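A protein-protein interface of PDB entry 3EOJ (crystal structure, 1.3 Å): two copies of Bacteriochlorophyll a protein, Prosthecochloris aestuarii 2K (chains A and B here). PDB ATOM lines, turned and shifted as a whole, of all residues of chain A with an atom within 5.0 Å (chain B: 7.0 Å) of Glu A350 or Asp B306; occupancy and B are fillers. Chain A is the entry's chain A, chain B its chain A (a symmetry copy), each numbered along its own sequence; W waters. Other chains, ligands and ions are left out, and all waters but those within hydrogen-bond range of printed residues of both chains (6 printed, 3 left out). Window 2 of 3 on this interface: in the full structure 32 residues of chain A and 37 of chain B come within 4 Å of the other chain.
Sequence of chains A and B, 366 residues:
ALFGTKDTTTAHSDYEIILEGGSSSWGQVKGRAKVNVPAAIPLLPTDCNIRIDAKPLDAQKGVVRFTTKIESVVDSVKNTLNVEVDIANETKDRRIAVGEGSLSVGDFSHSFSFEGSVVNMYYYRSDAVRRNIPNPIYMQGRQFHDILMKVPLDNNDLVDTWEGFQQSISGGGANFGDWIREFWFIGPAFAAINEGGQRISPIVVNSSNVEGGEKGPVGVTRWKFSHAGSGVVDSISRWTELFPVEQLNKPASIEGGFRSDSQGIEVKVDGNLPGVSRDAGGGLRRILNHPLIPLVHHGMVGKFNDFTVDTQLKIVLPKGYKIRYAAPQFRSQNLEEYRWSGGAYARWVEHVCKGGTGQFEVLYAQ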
ATOM      1  N   ASP A 306       6.346  10.696 -16.409  1.00  0.00           N
ATOM      2  CA  ASP A 306       6.021  10.567 -17.813  1.00  0.00           C
ATOM      3  C   ASP A 306       4.684  11.200 -18.062  1.00  0.00           C
ATOM      4  O   ASP A 306       3.777  11.054 -17.226  1.00  0.00           O
ATOM      5  CB  ASP A 306       5.877   9.072 -18.128  1.00  0.00           C
ATOM      6  CG  ASP A 306       7.206   8.374 -18.191  1.00  0.00           C
ATOM      7  OD1 ASP A 306       8.259   9.038 -18.131  1.00  0.00           O
ATOM      8  OD2 ASP A 306       7.156   7.129 -18.340  1.00  0.00           O
ATOM      9  N   PHE A 307       4.483  11.860 -19.190  1.00  0.00           N
ATOM     10  CA  PHE A 307       3.198  12.457 -19.501  1.00  0.00           C
ATOM     11  C   PHE A 307       2.975  12.483 -21.022  1.00  0.00           C
ATOM     12  O   PHE A 307       3.917  12.464 -21.801  1.00  0.00           O
ATOM     13  CB  PHE A 307       3.058  13.849 -18.941  1.00  0.00           C
ATOM     14  CG  PHE A 307       4.030  14.854 -19.549  1.00  0.00           C
ATOM     15  CD1 PHE A 307       3.715  15.625 -20.655  1.00  0.00           C
ATOM     16  CD2 PHE A 307       5.280  15.038 -18.954  1.00  0.00           C
ATOM     17  CE1 PHE A 307       4.637  16.547 -21.158  1.00  0.00           C
ATOM     18  CE2 PHE A 307       6.194  15.912 -19.487  1.00  0.00           C
ATOM     19  CZ  PHE A 307       5.896  16.670 -20.609  1.00  0.00           C
ATOM     20  N   VAL A 309       0.824  14.779 -23.927  1.00  0.00           N
ATOM     21  CA  VAL A 309       0.450  16.171 -24.153  1.00  0.00           C
ATOM     22  C   VAL A 309      -0.944  16.270 -24.776  1.00  0.00           C
ATOM     23  O   VAL A 309      -1.210  15.561 -25.785  1.00  0.00           O
ATOM     24  CB  VAL A 309       1.501  16.774 -25.118  1.00  0.00           C
ATOM     25  CG1 VAL A 309       1.048  18.106 -25.690  1.00  0.00           C
ATOM     26  CG2 VAL A 309       2.847  16.937 -24.424  1.00  0.00           C
ATOM     27  N   ALA A 346       3.024  19.158 -30.592  1.00  0.00           N
ATOM     28  CA  ALA A 346       2.928  18.464 -29.292  1.00  0.00           C
ATOM     29  C   ALA A 346       4.273  17.941 -28.824  1.00  0.00           C
ATOM     30  O   ALA A 346       4.577  17.932 -27.628  1.00  0.00           O
ATOM     31  CB  ALA A 346       1.929  17.308 -29.406  1.00  0.00           C
ATOM     32  N   ARG A 347       5.129  17.460 -29.757  1.00  0.00           N
ATOM     33  CA  ARG A 347       6.478  17.025 -29.368  1.00  0.00           C
ATOM     34  C   ARG A 347       7.315  18.224 -28.912  1.00  0.00           C
ATOM     35  O   ARG A 347       8.109  18.077 -27.995  1.00  0.00           O
ATOM     36  CB  ARG A 347       7.172  16.266 -30.468  1.00  0.00           C
ATOM     37  CG  ARG A 347       6.575  14.871 -30.682  1.00  0.00           C
ATOM     38  CD  ARG A 347       7.364  14.010 -31.699  1.00  0.00           C
ATOM     39  NE  ARG A 347       7.239  14.530 -33.047  1.00  0.00           N
ATOM     40  CZ  ARG A 347       6.262  14.287 -33.901  1.00  0.00           C
ATOM     41  NH1 ARG A 347       5.266  13.508 -33.569  1.00  0.00           N
ATOM     42  NH2 ARG A 347       6.301  14.861 -35.100  1.00  0.00           N
ATOM     43  N   TRP A 348       7.124  19.402 -29.517  1.00  0.00           N
ATOM     44  CA  TRP A 348       7.787  20.615 -29.045  1.00  0.00           C
ATOM     45  C   TRP A 348       7.321  20.986 -27.655  1.00  0.00           C
ATOM     46  O   TRP A 348       8.143  21.377 -26.810  1.00  0.00           O
ATOM     47  CB  TRP A 348       7.602  21.749 -30.099  1.00  0.00           C
ATOM     48  CG  TRP A 348       8.290  23.010 -29.633  1.00  0.00           C
ATOM     49  CD1 TRP A 348       9.588  23.362 -29.775  1.00  0.00           C
ATOM     50  CD2 TRP A 348       7.665  24.065 -28.907  1.00  0.00           C
ATOM     51  NE1 TRP A 348       9.829  24.571 -29.186  1.00  0.00           N
ATOM     52  CE2 TRP A 348       8.655  25.036 -28.644  1.00  0.00           C
ATOM     53  CE3 TRP A 348       6.364  24.338 -28.426  1.00  0.00           C
ATOM     54  CZ2 TRP A 348       8.389  26.214 -27.951  1.00  0.00           C
ATOM     55  CZ3 TRP A 348       6.107  25.504 -27.739  1.00  0.00           C
ATOM     56  CH2 TRP A 348       7.110  26.432 -27.504  1.00  0.00           C
ATOM     57  N   VAL A 349       5.996  20.890 -27.366  1.00  0.00           N
ATOM     58  CA  VAL A 349       5.495  21.200 -26.027  1.00  0.00           C
ATOM     59  C   VAL A 349       6.162  20.288 -25.010  1.00  0.00           C
ATOM     60  O   VAL A 349       6.642  20.713 -23.946  1.00  0.00           O
ATOM     61  CB  VAL A 349       3.979  21.090 -25.983  1.00  0.00           C
ATOM     62  CG1 VAL A 349       3.443  21.206 -24.550  1.00  0.00           C
ATOM     63  CG2 VAL A 349       3.313  22.148 -26.880  1.00  0.00           C
ATOM     64  N   GLU A 350       6.186  18.982 -25.307  1.00  0.00           N
ATOM     65  CA  GLU A 350       6.833  18.034 -24.377  1.00  0.00           C
ATOM     66  C   GLU A 350       8.288  18.436 -24.106  1.00  0.00           C
ATOM     67  O   GLU A 350       8.762  18.461 -22.977  1.00  0.00           O
ATOM     68  CB  GLU A 350       6.745  16.629 -24.969  1.00  0.00           C
ATOM     69  CG  GLU A 350       7.454  15.572 -24.140  1.00  0.00           C
ATOM     70  CD  GLU A 350       7.536  14.180 -24.768  1.00  0.00           C
ATOM     71  OE1 GLU A 350       7.280  14.035 -25.995  1.00  0.00           O
ATOM     72  OE2 GLU A 350       7.928  13.240 -24.074  1.00  0.00           O
ATOM     73  N   HIS A 351       8.984  18.762 -25.193  1.00  0.00           N
ATOM     74  CA  HIS A 351      10.379  19.153 -25.171  1.00  0.00           C
ATOM     75  C   HIS A 351      10.622  20.350 -24.276  1.00  0.00           C
ATOM     76  O   HIS A 351      11.484  20.299 -23.388  1.00  0.00           O
ATOM     77  CB  HIS A 351      10.815  19.414 -26.615  1.00  0.00           C
ATOM     78  CG  HIS A 351      12.144  20.063 -26.870  1.00  0.00           C
ATOM     79  ND1 HIS A 351      13.309  19.380 -27.129  1.00  0.00           N
ATOM     80  CD2 HIS A 351      12.488  21.361 -27.021  1.00  0.00           C
ATOM     81  CE1 HIS A 351      14.295  20.255 -27.402  1.00  0.00           C
ATOM     82  NE2 HIS A 351      13.818  21.484 -27.323  1.00  0.00           N
ATOM     83  N   VAL A 352       9.880  21.449 -24.493  1.00  0.00           N
ATOM     84  CA  VAL A 352      10.135  22.631 -23.684  1.00  0.00           C
ATOM     85  C   VAL A 352       9.697  22.474 -22.258  1.00  0.00           C
ATOM     86  O   VAL A 352      10.317  23.074 -21.391  1.00  0.00           O
ATOM     87  CB  VAL A 352       9.557  23.919 -24.307  1.00  0.00           C
ATOM     88  CG1 VAL A 352      10.184  24.178 -25.692  1.00  0.00           C
ATOM     89  CG2 VAL A 352       8.066  23.935 -24.348  1.00  0.00           C
ATOM     90  N   CYS A 353       8.663  21.660 -21.975  1.00  0.00           N
ATOM     91  CA  CYS A 353       8.275  21.424 -20.607  1.00  0.00           C
ATOM     92  C   CYS A 353       9.286  20.624 -19.788  1.00  0.00           C
ATOM     93  O   CYS A 353       9.271  20.672 -18.563  1.00  0.00           O
ATOM     94  CB  CYS A 353       6.914  20.711 -20.554  1.00  0.00           C
ATOM     95  SG  CYS A 353       5.523  21.757 -21.025  1.00  0.00           S
ATOM     96  N   LYS A 354      10.173  19.912 -20.466  1.00  0.00           N
ATOM     97  CA  LYS A 354      11.219  19.119 -19.859  1.00  0.00           C
ATOM     98  C   LYS A 354      12.570  19.856 -19.810  1.00  0.00           C
ATOM     99  O   LYS A 354      13.511  19.283 -19.256  1.00  0.00           O
ATOM    100  CB  LYS A 354      11.352  17.765 -20.579  1.00  0.00           C
ATOM    101  CG  LYS A 354      10.139  16.853 -20.352  1.00  0.00           C
ATOM    102  CD  LYS A 354      10.279  15.562 -21.182  1.00  0.00           C
ATOM    103  CE  LYS A 354       9.107  14.614 -20.915  1.00  0.00           C
ATOM    104  NZ  LYS A 354       9.093  13.388 -21.673  1.00  0.00           N
ATOM    105  N   THR B   8       4.510   7.525 -33.511  1.00  0.00           N
ATOM    106  CA  THR B   8       5.336   7.249 -32.327  1.00  0.00           C
ATOM    107  C   THR B   8       6.577   8.090 -32.306  1.00  0.00           C
ATOM    108  O   THR B   8       6.997   8.435 -33.420  1.00  0.00           O
ATOM    109  CB  THR B   8       5.732   5.744 -32.346  1.00  0.00           C
ATOM    110  OG1 THR B   8       6.661   5.510 -33.434  1.00  0.00           O
ATOM    111  CG2 THR B   8       4.454   4.930 -32.509  1.00  0.00           C
ATOM    112  N   THR B   9       7.125   8.359 -31.106  1.00  0.00           N
ATOM    113  CA  THR B   9       8.476   8.865 -31.220  1.00  0.00           C
ATOM    114  C   THR B   9       9.437   7.675 -31.155  1.00  0.00           C
ATOM    115  O   THR B   9       9.541   6.994 -30.124  1.00  0.00           O
ATOM    116  CB  THR B   9       8.717   9.848 -30.085  1.00  0.00           C
ATOM    117  OG1 THR B   9       7.696  10.865 -30.086  1.00  0.00           O
ATOM    118  CG2 THR B   9      10.051  10.515 -30.317  1.00  0.00           C
ATOM    119  N   THR B  10      10.106   7.449 -32.252  1.00  0.00           N
ATOM    120  CA  THR B  10      11.052   6.331 -32.370  1.00  0.00           C
ATOM    121  C   THR B  10      12.405   6.838 -32.800  1.00  0.00           C
ATOM    122  O   THR B  10      12.529   7.602 -33.784  1.00  0.00           O
ATOM    123  CB  THR B  10      10.524   5.291 -33.386  1.00  0.00           C
ATOM    124  OG1 THR B  10       9.237   4.796 -32.947  1.00  0.00           O
ATOM    125  CG2 THR B  10      11.479   4.107 -33.511  1.00  0.00           C
ATOM    126  N   VAL B  35      15.770  10.607 -35.644  1.00  0.00           N
ATOM    127  CA  VAL B  35      14.768  10.677 -34.579  1.00  0.00           C
ATOM    128  C   VAL B  35      13.901  11.886 -34.822  1.00  0.00           C
ATOM    129  O   VAL B  35      14.382  13.009 -35.067  1.00  0.00           O
ATOM    130  CB  VAL B  35      15.407  10.644 -33.184  1.00  0.00           C
ATOM    131  CG1 VAL B  35      16.385  11.732 -32.982  1.00  0.00           C
ATOM    132  CG2 VAL B  35      14.364  10.580 -32.066  1.00  0.00           C
ATOM    133  N   ASN B  36      12.579  11.683 -34.726  1.00  0.00           N
ATOM    134  CA  ASN B  36      11.589  12.702 -35.031  1.00  0.00           C
ATOM    135  C   ASN B  36      11.250  13.554 -33.812  1.00  0.00           C
ATOM    136  O   ASN B  36      10.078  13.583 -33.363  1.00  0.00           O
ATOM    137  CB  ASN B  36      10.330  12.008 -35.544  1.00  0.00           C
ATOM    138  CG  ASN B  36       9.571  11.094 -34.581  1.00  0.00           C
ATOM    139  OD1 ASN B  36      10.279  10.351 -33.840  1.00  0.00           O
ATOM    140  ND2 ASN B  36       8.245  11.037 -34.457  1.00  0.00           N
ATOM    141  N   VAL B  37      12.240  14.230 -33.277  1.00  0.00           N
ATOM    142  CA  VAL B  37      12.118  15.167 -32.177  1.00  0.00           C
ATOM    143  C   VAL B  37      12.808  16.462 -32.525  1.00  0.00           C
ATOM    144  O   VAL B  37      13.719  16.484 -33.340  1.00  0.00           O
ATOM    145  CB  VAL B  37      12.715  14.604 -30.870  1.00  0.00           C
ATOM    146  CG1 VAL B  37      11.983  13.323 -30.499  1.00  0.00           C
ATOM    147  CG2 VAL B  37      14.206  14.383 -31.027  1.00  0.00           C
ATOM    148  N   GLY B 302      19.366  14.722 -24.107  1.00  0.00           N
ATOM    149  CA  GLY B 302      18.631  13.517 -24.484  1.00  0.00           C
ATOM    150  C   GLY B 302      17.398  13.171 -23.702  1.00  0.00           C
ATOM    151  O   GLY B 302      16.808  12.101 -23.985  1.00  0.00           O
ATOM    152  N   LYS B 303      16.963  13.993 -22.766  1.00  0.00           N
ATOM    153  CA  LYS B 303      15.832  13.686 -21.895  1.00  0.00           C
ATOM    154  C   LYS B 303      14.557  14.468 -22.173  1.00  0.00           C
ATOM    155  O   LYS B 303      13.654  14.481 -21.337  1.00  0.00           O
ATOM    156  CB  LYS B 303      16.213  13.893 -20.411  1.00  0.00           C
ATOM    157  CG  LYS B 303      17.442  13.094 -19.939  1.00  0.00           C
ATOM    158  CD  LYS B 303      17.628  13.307 -18.421  1.00  0.00           C
ATOM    159  CE  LYS B 303      18.869  12.769 -17.833  1.00  0.00           C
ATOM    160  NZ  LYS B 303      20.048  13.533 -18.343  1.00  0.00           N
ATOM    161  N   PHE B 304      14.478  15.147 -23.320  1.00  0.00           N
ATOM    162  CA  PHE B 304      13.359  16.066 -23.543  1.00  0.00           C
ATOM    163  C   PHE B 304      12.186  15.474 -24.299  1.00  0.00           C
ATOM    164  O   PHE B 304      11.136  16.131 -24.388  1.00  0.00           O
ATOM    165  CB  PHE B 304      13.841  17.329 -24.262  1.00  0.00           C
ATOM    166  CG  PHE B 304      14.957  18.088 -23.585  1.00  0.00           C
ATOM    167  CD1 PHE B 304      14.955  18.323 -22.217  1.00  0.00           C
ATOM    168  CD2 PHE B 304      16.008  18.586 -24.300  1.00  0.00           C
ATOM    169  CE1 PHE B 304      15.953  19.077 -21.635  1.00  0.00           C
ATOM    170  CE2 PHE B 304      17.022  19.339 -23.734  1.00  0.00           C
ATOM    171  CZ  PHE B 304      16.985  19.582 -22.381  1.00  0.00           C
ATOM    172  N   ASN B 305      12.277  14.268 -24.820  1.00  0.00           N
ATOM    173  CA  ASN B 305      11.138  13.610 -25.459  1.00  0.00           C
ATOM    174  C   ASN B 305      11.198  12.116 -25.229  1.00  0.00           C
ATOM    175  O   ASN B 305      12.221  11.497 -25.420  1.00  0.00           O
ATOM    176  CB  ASN B 305      11.070  13.818 -26.965  1.00  0.00           C
ATOM    177  CG  ASN B 305      10.689  15.204 -27.401  1.00  0.00           C
ATOM    178  OD1 ASN B 305      11.484  16.058 -27.748  1.00  0.00           O
ATOM    179  ND2 ASN B 305       9.387  15.503 -27.403  1.00  0.00           N
ATOM    180  N   ASP B 306      10.056  11.519 -24.894  1.00  0.00           N
ATOM    181  CA  ASP B 306      10.003  10.082 -24.740  1.00  0.00           C
ATOM    182  C   ASP B 306      10.273   9.440 -26.068  1.00  0.00           C
ATOM    183  O   ASP B 306       9.795   9.946 -27.097  1.00  0.00           O
ATOM    184  CB  ASP B 306       8.570   9.704 -24.341  1.00  0.00           C
ATOM    185  CG  ASP B 306       8.270  10.045 -22.909  1.00  0.00           C
ATOM    186  OD1 ASP B 306       9.183  10.447 -22.162  1.00  0.00           O
ATOM    187  OD2 ASP B 306       7.083   9.860 -22.546  1.00  0.00           O
ATOM    188  N   PHE B 307      10.978   8.322 -26.113  1.00  0.00           N
ATOM    189  CA  PHE B 307      11.235   7.638 -27.365  1.00  0.00           C
ATOM    190  C   PHE B 307      11.370   6.124 -27.130  1.00  0.00           C
ATOM    191  O   PHE B 307      11.696   5.680 -26.037  1.00  0.00           O
ATOM    192  CB  PHE B 307      12.465   8.157 -28.065  1.00  0.00           C
ATOM    193  CG  PHE B 307      13.758   7.907 -27.295  1.00  0.00           C
ATOM    194  CD1 PHE B 307      14.534   6.776 -27.483  1.00  0.00           C
ATOM    195  CD2 PHE B 307      14.204   8.869 -26.386  1.00  0.00           C
ATOM    196  CE1 PHE B 307      15.722   6.609 -26.765  1.00  0.00           C
ATOM    197  CE2 PHE B 307      15.349   8.669 -25.654  1.00  0.00           C
ATOM    198  CZ  PHE B 307      16.119   7.528 -25.817  1.00  0.00           C
ATOM    199  N   THR B 308      11.063   5.411 -28.238  1.00  0.00           N
ATOM    200  CA  THR B 308      11.277   3.994 -28.395  1.00  0.00           C
ATOM    201  C   THR B 308      12.558   3.791 -29.182  1.00  0.00           C
ATOM    202  O   THR B 308      12.822   4.575 -30.080  1.00  0.00           O
ATOM    203  CB  THR B 308      10.074   3.358 -29.134  1.00  0.00           C
ATOM    204  OG1 THR B 308       8.859   3.655 -28.403  1.00  0.00           O
ATOM    205  CG2 THR B 308      10.193   1.849 -29.231  1.00  0.00           C
ATOM    206  N   LYS B 354      20.360   9.081 -22.915  1.00  0.00           N
ATOM    207  CA  LYS B 354      19.817   9.968 -21.909  1.00  0.00           C
ATOM    208  C   LYS B 354      20.881  10.455 -20.910  1.00  0.00           C
ATOM    209  O   LYS B 354      20.526  11.263 -20.049  1.00  0.00           O
ATOM    210  CB  LYS B 354      18.640   9.295 -21.181  1.00  0.00           C
ATOM    211  CG  LYS B 354      17.414   9.109 -22.085  1.00  0.00           C
ATOM    212  CD  LYS B 354      16.311   8.335 -21.336  1.00  0.00           C
ATOM    213  CE  LYS B 354      15.056   8.200 -22.204  1.00  0.00           C
ATOM    214  NZ  LYS B 354      13.966   7.447 -21.635  1.00  0.00           N
HETATM  215  O   HOH W   1       7.657  11.687 -27.301  1.00  0.00           O
HETATM  216  O   HOH W   2       8.645  16.291 -34.463  1.00  0.00           O
HETATM  217  O   HOH W   3       5.007  11.279 -31.084  1.00  0.00           O
HETATM  218  O   HOH W   4      14.070  16.641 -27.896  1.00  0.00           O
HETATM  219  O   HOH W   5       6.854  12.075 -20.962  1.00  0.00           O
HETATM  220  O   HOH W   6       6.981  12.028 -36.973  1.00  0.00           O
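O of Asn B36 sits at hydrogen-bond distance from NE of Arg A347 (3.0 Å).
The backbone NH of Asp B306 lies within hydrogen-bond range of the side-chain carboxylate of Glu A350 (2.9 Å).
ND2 of Asn B305 lies within hydrogen-bond range of O of Arg A347, 2.9 Å away.
N of His A351 lies close to O of Phe B304 (3.5 Å).
OE1 of Glu A350 lies within hydrogen-bond range of ND2 of Asn B305 (2.9 Å).
The side-chain carboxylate (OD1) of Asp B306 is in salt-bridge range of the side-chain amino group (NZ) of Lys A354, 3.0 Å away.
The side-chain amino group (NZ) of Lys B303 sits at hydrogen-bond distance from the backbone carbonyl oxygen (O) of Lys B354 (2.9 Å).
The backbone carbonyl oxygen of Thr B9 sits at hydrogen-bond distance from the backbone NH of Thr B308 (2.9 Å).
The side-chain amino group (NZ) of Lys A354 lies within salt-bridge range of the side-chain carboxylate (OE2) of Glu A350 (2.7 Å).
The backbone NH of Thr B10 lies within hydrogen-bond range of the side-chain amide oxygen of Asn B36 (3.3 Å).
O of Thr B8 sits at hydrogen-bond distance from ND2 of Asn B36.
CD of Arg A347 touches OG1 of Thr B9 (3.6 Å).
Glu A350 touches Phe B304 (O to O, 3.6 Å).
CB of His A351 touches OD1 of Asn B305, at 3.6 Å.
CD of Lys A354 touches O of Lys B303, at 3.5 Å.
Lys A354 touches Phe B304.
Of the printed residues of chain B, Arg A347 touches Thr B9 (3.6 Å), Asn B36 (3.0 Å) and Asn B305 (2.9 Å).
Of the printed residues of chain B, Glu A350 touches Phe B304 (3.6 Å), Asn B305 (2.9 Å) and Asp B306 (2.9 Å).
Of the printed residues of chain A, Lys B303 touches Lys A354 (3.5 Å).
Printed residues of chain A within 4 Å of Asp B306: Glu A350 (2.9 Å) and Lys A354 (3.0 Å).
The nearest printed residue of chain B that does not touch Glu A350 is Thr B9 (5.2 Å).
Of the 14 printed residues of chain B, 6 touch a printed residue of chain A.
Of the 12 printed residues of chain A, 4 touch a printed residue of chain B.
Along chain A the printed residues that touch a printed residue of chain B span positions 347 to 354.
Among the printed residues, 11 pairs touch across the chains.
Lys A354 touches Asp B306, but with the chains exchanged Asp A306 does not touch Lys B354 (6.9 Å).
Of the 11 pairs that touch across the chains among the printed residues, none has its exchanged pair printed and touching as well.
Water W4 bridges the side-chain amide oxygen (OD1) of Asn B305 and a ring nitrogen (ND1) of His A351.
Water W2 lies within hydrogen-bond range of NE of Arg A347 and O of Asn B36.
Water W5 lies within hydrogen-bond range of the side-chain amino group of Lys A354 (2.7 Å), the side-chain carboxylate of Asp B306 (2.7 Å), the backbone NH of Phe A307 (3.0 Å) and the side-chain carboxylate of Glu A350 (3.5 Å).
Water W1 lies within hydrogen-bond range of the side-chain carboxylate (OE1) of Glu A350 (2.7 Å), the backbone carbonyl oxygen (O) of Asp B306 (2.8 Å) and the side-chain hydroxyl (OG1) of Thr B9 (2.9 Å).
Water W3 lies within hydrogen-bond range of the side-chain hydroxyl (OG1) of Thr B9 and the guanidinium group (NH1) of Arg A347.
Water W6 bridges ND2 of Asn B36 (3.0 Å) and NH2 of Arg A347 (3.5 Å).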
